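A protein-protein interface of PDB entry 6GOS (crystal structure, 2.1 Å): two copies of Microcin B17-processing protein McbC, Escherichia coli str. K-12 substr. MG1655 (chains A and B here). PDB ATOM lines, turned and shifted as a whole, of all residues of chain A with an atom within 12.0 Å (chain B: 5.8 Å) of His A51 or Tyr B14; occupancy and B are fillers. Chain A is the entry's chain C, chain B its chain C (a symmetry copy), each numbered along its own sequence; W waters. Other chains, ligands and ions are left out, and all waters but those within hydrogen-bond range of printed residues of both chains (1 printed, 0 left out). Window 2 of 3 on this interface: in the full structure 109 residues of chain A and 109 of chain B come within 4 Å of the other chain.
Ala A46 touches Tyr B14 (O to CD1, 3.6 Å).
Ala A46 touches Phe B200 (CB to O, 3.3 Å).
Tyr B14 touches Val A47.
Val A47 touches Phe B200 (CG2 to CD2, 3.7 Å).
CD of Pro A48 touches CE1 of Tyr B14, 3.4 Å away.
Glu B10 touches Phe A55.
Phe A55 touches Val B11 (CE1 to N, 3.6 Å).
CZ of Phe A55 touches CE2 of Tyr B14, 3.7 Å away.
CD1 of Phe A55 touches CE2 of Phe B200, 3.5 Å away.
The side-chain carboxylate (OE1) of Glu B10 lies within salt-bridge range of the side-chain amino group (NZ) of Lys A54, at 3.4 Å.
The side-chain hydroxyl (OH) of Tyr B14 lies within hydrogen-bond range of a ring nitrogen (ND1) of His A51, at 3.2 Å.
The backbone carbonyl oxygen (O) of Val A47 sits at hydrogen-bond distance from the side-chain hydroxyl (OG) of Ser A45 (2.7 Å).
Of the 8 printed residues of chain B, 4 touch a printed residue of chain A.
Hydrophobic or aromatic side chains of chain B within 4 Å of the printed part of chain A: Val B11, Tyr B14 and Phe B200.
Of the 16 printed residues of chain A, 6 touch a printed residue of chain B.
Hydrophobic or aromatic side chains of chain A within 4 Å of the printed part of chain B: Ala A46, Val A47, Pro A48, His A51 and Phe A55.
Among the printed residues, 11 pairs touch across the chains.
No position is printed for both chains.
Of the 11 pairs that touch across the chains among the printed residues, none has its exchanged pair printed and touching as well.
Water W1 bridges the side-chain hydroxyl of Tyr B14 (2.5 Å) and the side-chain amino group of Lys A54 (2.7 Å).
Val A44 touches none of the printed residues of chain B.
Printed residues of chain B within 4 Å of Ala A46: Tyr B14 and Phe B200.
Of chain B, only Tyr B14 comes within 4 Å of His A51.
Of the printed residues of chain A, Glu B10 touches Lys A54 (3.4 Å) and Phe A55 (3.5 Å).
Of chain A, only Phe A55 comes within 4 Å of Val B11.
No residue of chain A comes within 4 Å of His B13.
Of chain A, only Ala A46 (3.6 Å), Val A47 (3.9 Å), Pro A48 (3.4 Å), His A51 (3.2 Å) and Phe A55 (3.7 Å) come within 4 Å of Tyr B14.
No residue of chain A comes within 4 Å of Thr B15.
Phe B200 touches just these residues of chain A: Ala A46 (3.3 Å), Val A47 (3.7 Å) and Phe A55 (3.5 Å).
The nearest printed residue of chain B that does not touch Phe A55 is Thr B12 (6.0 Å).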
ATOM      1  N   PHE A  43     -21.049   7.076 -26.321  1.00  0.00           N
ATOM      2  CA  PHE A  43     -20.198   7.380 -25.178  1.00  0.00           C
ATOM      3  C   PHE A  43     -19.464   6.134 -24.720  1.00  0.00           C
ATOM      4  O   PHE A  43     -19.795   4.997 -25.126  1.00  0.00           O
ATOM      5  CB  PHE A  43     -20.990   8.029 -24.031  1.00  0.00           C
ATOM      6  CG  PHE A  43     -21.903   7.080 -23.308  1.00  0.00           C
ATOM      7  CD1 PHE A  43     -23.112   6.699 -23.873  1.00  0.00           C
ATOM      8  CD2 PHE A  43     -21.563   6.584 -22.064  1.00  0.00           C
ATOM      9  CE1 PHE A  43     -23.944   5.822 -23.216  1.00  0.00           C
ATOM     10  CE2 PHE A  43     -22.392   5.698 -21.400  1.00  0.00           C
ATOM     11  CZ  PHE A  43     -23.587   5.321 -21.974  1.00  0.00           C
ATOM     12  N   VAL A  44     -18.434   6.369 -23.916  1.00  0.00           N
ATOM     13  CA  VAL A  44     -17.555   5.323 -23.416  1.00  0.00           C
ATOM     14  C   VAL A  44     -17.713   5.150 -21.893  1.00  0.00           C
ATOM     15  O   VAL A  44     -17.864   4.023 -21.415  1.00  0.00           O
ATOM     16  CB  VAL A  44     -16.066   5.595 -23.763  1.00  0.00           C
ATOM     17  CG1 VAL A  44     -15.207   4.403 -23.373  1.00  0.00           C
ATOM     18  CG2 VAL A  44     -15.889   5.863 -25.237  1.00  0.00           C
ATOM     19  N   SER A  45     -17.637   6.264 -21.158  1.00  0.00           N
ATOM     20  CA  SER A  45     -17.624   6.267 -19.704  1.00  0.00           C
ATOM     21  C   SER A  45     -19.028   6.400 -19.174  1.00  0.00           C
ATOM     22  O   SER A  45     -19.706   7.349 -19.476  1.00  0.00           O
ATOM     23  CB  SER A  45     -16.781   7.439 -19.175  1.00  0.00           C
ATOM     24  OG  SER A  45     -16.778   7.456 -17.761  1.00  0.00           O
ATOM     25  N   ALA A  46     -19.447   5.438 -18.361  1.00  0.00           N
ATOM     26  CA  ALA A  46     -20.713   5.516 -17.663  1.00  0.00           C
ATOM     27  C   ALA A  46     -20.646   6.499 -16.479  1.00  0.00           C
ATOM     28  O   ALA A  46     -21.678   6.877 -15.934  1.00  0.00           O
ATOM     29  CB  ALA A  46     -21.128   4.126 -17.218  1.00  0.00           C
ATOM     30  N   VAL A  47     -19.449   6.937 -16.099  1.00  0.00           N
ATOM     31  CA  VAL A  47     -19.291   7.931 -15.054  1.00  0.00           C
ATOM     32  C   VAL A  47     -19.038   9.297 -15.685  1.00  0.00           C
ATOM     33  O   VAL A  47     -18.157   9.411 -16.514  1.00  0.00           O
ATOM     34  CB  VAL A  47     -18.083   7.580 -14.171  1.00  0.00           C
ATOM     35  CG1 VAL A  47     -17.909   8.604 -13.041  1.00  0.00           C
ATOM     36  CG2 VAL A  47     -18.226   6.167 -13.620  1.00  0.00           C
ATOM     37  N   PRO A  48     -19.775  10.351 -15.265  1.00  0.00           N
ATOM     38  CA  PRO A  48     -19.479  11.708 -15.756  1.00  0.00           C
ATOM     39  C   PRO A  48     -18.050  12.131 -15.457  1.00  0.00           C
ATOM     40  O   PRO A  48     -17.540  11.824 -14.383  1.00  0.00           O
ATOM     41  CB  PRO A  48     -20.468  12.584 -14.987  1.00  0.00           C
ATOM     42  CG  PRO A  48     -21.609  11.686 -14.686  1.00  0.00           C
ATOM     43  CD  PRO A  48     -21.000  10.331 -14.443  1.00  0.00           C
ATOM     44  N   LEU A  49     -17.418  12.819 -16.408  1.00  0.00           N
ATOM     45  CA  LEU A  49     -15.999  13.208 -16.302  1.00  0.00           C
ATOM     46  C   LEU A  49     -15.705  14.004 -15.024  1.00  0.00           C
ATOM     47  O   LEU A  49     -14.635  13.855 -14.444  1.00  0.00           O
ATOM     48  CB  LEU A  49     -15.569  14.009 -17.548  1.00  0.00           C
ATOM     49  CG  LEU A  49     -14.151  14.623 -17.626  1.00  0.00           C
ATOM     50  CD1 LEU A  49     -13.068  13.551 -17.733  1.00  0.00           C
ATOM     51  CD2 LEU A  49     -14.053  15.610 -18.790  1.00  0.00           C
ATOM     52  N   ALA A  50     -16.663  14.827 -14.591  1.00  0.00           N
ATOM     53  CA  ALA A  50     -16.547  15.590 -13.344  1.00  0.00           C
ATOM     54  C   ALA A  50     -16.457  14.737 -12.077  1.00  0.00           C
ATOM     55  O   ALA A  50     -15.920  15.192 -11.093  1.00  0.00           O
ATOM     56  CB  ALA A  50     -17.714  16.557 -13.208  1.00  0.00           C
ATOM     57  N   HIS A  51     -17.016  13.534 -12.076  1.00  0.00           N
ATOM     58  CA  HIS A  51     -16.942  12.669 -10.903  1.00  0.00           C
ATOM     59  C   HIS A  51     -15.854  11.588 -11.017  1.00  0.00           C
ATOM     60  O   HIS A  51     -15.666  10.837 -10.067  1.00  0.00           O
ATOM     61  CB  HIS A  51     -18.304  12.025 -10.639  1.00  0.00           C
ATOM     62  CG  HIS A  51     -19.372  13.002 -10.265  1.00  0.00           C
ATOM     63  ND1 HIS A  51     -20.615  13.010 -10.862  1.00  0.00           N
ATOM     64  CD2 HIS A  51     -19.386  14.002  -9.350  1.00  0.00           C
ATOM     65  CE1 HIS A  51     -21.347  13.975 -10.336  1.00  0.00           C
ATOM     66  NE2 HIS A  51     -20.628  14.586  -9.412  1.00  0.00           N
ATOM     67  N   LEU A  52     -15.141  11.508 -12.145  1.00  0.00           N
ATOM     68  CA  LEU A  52     -14.128  10.454 -12.351  1.00  0.00           C
ATOM     69  C   LEU A  52     -12.982  10.532 -11.353  1.00  0.00           C
ATOM     70  O   LEU A  52     -12.532   9.515 -10.846  1.00  0.00           O
ATOM     71  CB  LEU A  52     -13.546  10.476 -13.779  1.00  0.00           C
ATOM     72  CG  LEU A  52     -14.316   9.783 -14.895  1.00  0.00           C
ATOM     73  CD1 LEU A  52     -13.569   9.924 -16.213  1.00  0.00           C
ATOM     74  CD2 LEU A  52     -14.515   8.299 -14.597  1.00  0.00           C
ATOM     75  N   GLU A  53     -12.541  11.740 -11.043  1.00  0.00           N
ATOM     76  CA  GLU A  53     -11.347  11.941 -10.231  1.00  0.00           C
ATOM     77  C   GLU A  53     -11.408  11.238  -8.865  1.00  0.00           C
ATOM     78  O   GLU A  53     -10.392  10.726  -8.385  1.00  0.00           O
ATOM     79  CB  GLU A  53     -11.082  13.454 -10.081  1.00  0.00           C
ATOM     80  CG  GLU A  53      -9.684  13.816  -9.593  1.00  0.00           C
ATOM     81  CD  GLU A  53      -9.566  13.952  -8.080  1.00  0.00           C
ATOM     82  OE1 GLU A  53     -10.564  13.714  -7.358  1.00  0.00           O
ATOM     83  OE2 GLU A  53      -8.462  14.313  -7.603  1.00  0.00           O
ATOM     84  N   LYS A  54     -12.597  11.187  -8.258  1.00  0.00           N
ATOM     85  CA  LYS A  54     -12.783  10.518  -6.967  1.00  0.00           C
ATOM     86  C   LYS A  54     -12.611   8.973  -7.054  1.00  0.00           C
ATOM     87  O   LYS A  54     -12.456   8.319  -6.044  1.00  0.00           O
ATOM     88  CB  LYS A  54     -14.140  10.910  -6.329  1.00  0.00           C
ATOM     89  CG  LYS A  54     -15.293   9.910  -6.496  1.00  0.00           C
ATOM     90  CD  LYS A  54     -16.596  10.405  -5.862  1.00  0.00           C
ATOM     91  CE  LYS A  54     -17.560  11.010  -6.870  1.00  0.00           C
ATOM     92  NZ  LYS A  54     -18.858  11.367  -6.217  1.00  0.00           N
ATOM     93  N   PHE A  55     -12.670   8.393  -8.249  1.00  0.00           N
ATOM     94  CA  PHE A  55     -12.515   6.949  -8.429  1.00  0.00           C
ATOM     95  C   PHE A  55     -11.100   6.533  -8.834  1.00  0.00           C
ATOM     96  O   PHE A  55     -10.759   5.358  -8.755  1.00  0.00           O
ATOM     97  CB  PHE A  55     -13.517   6.438  -9.466  1.00  0.00           C
ATOM     98  CG  PHE A  55     -14.942   6.649  -9.068  1.00  0.00           C
ATOM     99  CD1 PHE A  55     -15.539   5.834  -8.104  1.00  0.00           C
ATOM    100  CD2 PHE A  55     -15.695   7.680  -9.626  1.00  0.00           C
ATOM    101  CE1 PHE A  55     -16.859   6.046  -7.711  1.00  0.00           C
ATOM    102  CE2 PHE A  55     -17.029   7.881  -9.249  1.00  0.00           C
ATOM    103  CZ  PHE A  55     -17.607   7.079  -8.282  1.00  0.00           C
ATOM    104  N   GLU A  56     -10.275   7.492  -9.239  1.00  0.00           N
ATOM    105  CA  GLU A  56      -8.972   7.197  -9.830  1.00  0.00           C
ATOM    106  C   GLU A  56      -7.852   7.099  -8.805  1.00  0.00           C
ATOM    107  O   GLU A  56      -7.743   7.932  -7.893  1.00  0.00           O
ATOM    108  CB  GLU A  56      -8.638   8.272 -10.841  1.00  0.00           C
ATOM    109  CG  GLU A  56      -9.570   8.217 -12.037  1.00  0.00           C
ATOM    110  CD  GLU A  56      -9.387   9.379 -12.968  1.00  0.00           C
ATOM    111  OE1 GLU A  56      -8.587  10.298 -12.666  1.00  0.00           O
ATOM    112  OE2 GLU A  56     -10.061   9.390 -14.009  1.00  0.00           O
ATOM    113  N   ASN A  57      -7.021   6.074  -8.951  1.00  0.00           N
ATOM    114  CA  ASN A  57      -5.886   5.872  -8.051  1.00  0.00           C
ATOM    115  C   ASN A  57      -6.294   5.867  -6.570  1.00  0.00           C
ATOM    116  O   ASN A  57      -5.737   6.613  -5.771  1.00  0.00           O
ATOM    117  CB  ASN A  57      -4.795   6.942  -8.293  1.00  0.00           C
ATOM    118  CG  ASN A  57      -4.321   6.961  -9.730  1.00  0.00           C
ATOM    119  OD1 ASN A  57      -3.939   5.931 -10.270  1.00  0.00           O
ATOM    120  ND2 ASN A  57      -4.373   8.125 -10.358  1.00  0.00           N
ATOM    121  N   LYS A  58      -7.255   5.017  -6.229  1.00  0.00           N
ATOM    122  CA  LYS A  58      -7.696   4.851  -4.851  1.00  0.00           C
ATOM    123  C   LYS A  58      -7.479   3.433  -4.340  1.00  0.00           C
ATOM    124  O   LYS A  58      -7.038   2.558  -5.080  1.00  0.00           O
ATOM    125  CB  LYS A  58      -9.163   5.254  -4.741  1.00  0.00           C
ATOM    126  CG  LYS A  58      -9.423   6.733  -5.048  1.00  0.00           C
ATOM    127  CD  LYS A  58      -8.662   7.687  -4.122  1.00  0.00           C
ATOM    128  CE  LYS A  58      -9.123   9.131  -4.236  1.00  0.00           C
ATOM    129  NZ  LYS A  58      -8.959   9.623  -5.625  1.00  0.00           N
ATOM    130  N   GLU B  10     -19.908   4.589  -3.481  1.00  0.00           N
ATOM    131  CA  GLU B  10     -19.765   5.562  -4.592  1.00  0.00           C
ATOM    132  C   GLU B  10     -19.734   4.852  -5.929  1.00  0.00           C
ATOM    133  O   GLU B  10     -20.313   5.329  -6.912  1.00  0.00           O
ATOM    134  CB  GLU B  10     -18.458   6.359  -4.489  1.00  0.00           C
ATOM    135  CG  GLU B  10     -18.295   7.211  -3.242  1.00  0.00           C
ATOM    136  CD  GLU B  10     -19.099   8.503  -3.258  1.00  0.00           C
ATOM    137  OE1 GLU B  10     -19.831   8.792  -4.242  1.00  0.00           O
ATOM    138  OE2 GLU B  10     -18.988   9.241  -2.251  1.00  0.00           O
ATOM    139  N   VAL B  11     -19.003   3.740  -5.966  1.00  0.00           N
ATOM    140  CA  VAL B  11     -18.892   2.927  -7.161  1.00  0.00           C
ATOM    141  C   VAL B  11     -20.244   2.359  -7.595  1.00  0.00           C
ATOM    142  O   VAL B  11     -20.581   2.417  -8.774  1.00  0.00           O
ATOM    143  CB  VAL B  11     -17.848   1.795  -6.992  1.00  0.00           C
ATOM    144  CG1 VAL B  11     -17.885   0.828  -8.175  1.00  0.00           C
ATOM    145  CG2 VAL B  11     -16.463   2.390  -6.870  1.00  0.00           C
ATOM    146  N   THR B  12     -21.016   1.828  -6.650  1.00  0.00           N
ATOM    147  CA  THR B  12     -22.282   1.156  -6.996  1.00  0.00           C
ATOM    148  C   THR B  12     -23.336   2.107  -7.566  1.00  0.00           C
ATOM    149  O   THR B  12     -24.240   1.674  -8.293  1.00  0.00           O
ATOM    150  CB  THR B  12     -22.863   0.331  -5.824  1.00  0.00           C
ATOM    151  OG1 THR B  12     -23.768  -0.635  -6.353  1.00  0.00           O
ATOM    152  CG2 THR B  12     -23.572   1.231  -4.712  1.00  0.00           C
ATOM    153  N   HIS B  13     -23.184   3.398  -7.279  1.00  0.00           N
ATOM    154  CA  HIS B  13     -24.058   4.400  -7.824  1.00  0.00           C
ATOM    155  C   HIS B  13     -24.126   4.324  -9.357  1.00  0.00           C
ATOM    156  O   HIS B  13     -25.136   4.687  -9.922  1.00  0.00           O
ATOM    157  CB  HIS B  13     -23.614   5.794  -7.352  1.00  0.00           C
ATOM    158  CG  HIS B  13     -24.660   6.841  -7.492  1.00  0.00           C
ATOM    159  ND1 HIS B  13     -25.959   6.655  -7.069  1.00  0.00           N
ATOM    160  CD2 HIS B  13     -24.600   8.103  -7.990  1.00  0.00           C
ATOM    161  CE1 HIS B  13     -26.660   7.748  -7.321  1.00  0.00           C
ATOM    162  NE2 HIS B  13     -25.857   8.644  -7.870  1.00  0.00           N
ATOM    163  N   TYR B  14     -23.068   3.841 -10.016  1.00  0.00           N
ATOM    164  CA  TYR B  14     -23.019   3.780 -11.479  1.00  0.00           C
ATOM    165  C   TYR B  14     -23.216   2.369 -12.053  1.00  0.00           C
ATOM    166  O   TYR B  14     -23.107   2.185 -13.257  1.00  0.00           O
ATOM    167  CB  TYR B  14     -21.694   4.379 -11.973  1.00  0.00           C
ATOM    168  CG  TYR B  14     -21.563   5.856 -11.628  1.00  0.00           C
ATOM    169  CD1 TYR B  14     -22.208   6.827 -12.379  1.00  0.00           C
ATOM    170  CD2 TYR B  14     -20.856   6.264 -10.502  1.00  0.00           C
ATOM    171  CE1 TYR B  14     -22.134   8.179 -12.024  1.00  0.00           C
ATOM    172  CE2 TYR B  14     -20.770   7.598 -10.148  1.00  0.00           C
ATOM    173  CZ  TYR B  14     -21.405   8.550 -10.909  1.00  0.00           C
ATOM    174  OH  TYR B  14     -21.294   9.858 -10.531  1.00  0.00           O
ATOM    175  N   THR B  15     -23.496   1.376 -11.208  1.00  0.00           N
ATOM    176  CA  THR B  15     -23.545  -0.028 -11.647  1.00  0.00           C
ATOM    177  C   THR B  15     -24.785  -0.321 -12.495  1.00  0.00           C
ATOM    178  O   THR B  15     -25.917   0.004 -12.120  1.00  0.00           O
ATOM    179  CB  THR B  15     -23.469  -0.988 -10.447  1.00  0.00           C
ATOM    180  OG1 THR B  15     -22.132  -0.994  -9.969  1.00  0.00           O
ATOM    181  CG2 THR B  15     -23.900  -2.461 -10.810  1.00  0.00           C
ATOM    182  N   ASP B  16     -24.548  -0.943 -13.647  1.00  0.00           N
ATOM    183  CA  ASP B  16     -25.628  -1.492 -14.448  1.00  0.00           C
ATOM    184  C   ASP B  16     -25.854  -2.922 -13.962  1.00  0.00           C
ATOM    185  O   ASP B  16     -24.994  -3.793 -14.143  1.00  0.00           O
ATOM    186  CB  ASP B  16     -25.287  -1.473 -15.931  1.00  0.00           C
ATOM    187  CG  ASP B  16     -26.449  -2.001 -16.809  1.00  0.00           C
ATOM    188  OD1 ASP B  16     -27.285  -2.802 -16.327  1.00  0.00           O
ATOM    189  OD2 ASP B  16     -26.537  -1.612 -17.985  1.00  0.00           O
ATOM    190  N   PHE B 200     -18.002  -0.604 -13.516  1.00  0.00           N
ATOM    191  CA  PHE B 200     -18.820   0.608 -13.409  1.00  0.00           C
ATOM    192  C   PHE B 200     -18.644   1.654 -14.487  1.00  0.00           C
ATOM    193  O   PHE B 200     -19.629   2.285 -14.881  1.00  0.00           O
ATOM    194  CB  PHE B 200     -18.794   1.223 -12.003  1.00  0.00           C
ATOM    195  CG  PHE B 200     -17.595   2.061 -11.683  1.00  0.00           C
ATOM    196  CD1 PHE B 200     -16.321   1.528 -11.692  1.00  0.00           C
ATOM    197  CD2 PHE B 200     -17.764   3.363 -11.252  1.00  0.00           C
ATOM    198  CE1 PHE B 200     -15.240   2.294 -11.325  1.00  0.00           C
ATOM    199  CE2 PHE B 200     -16.681   4.134 -10.890  1.00  0.00           C
ATOM    200  CZ  PHE B 200     -15.423   3.609 -10.934  1.00  0.00           C
HETATM  201  O   HOH W   1     -20.390  10.269  -8.193  1.00  0.00           O
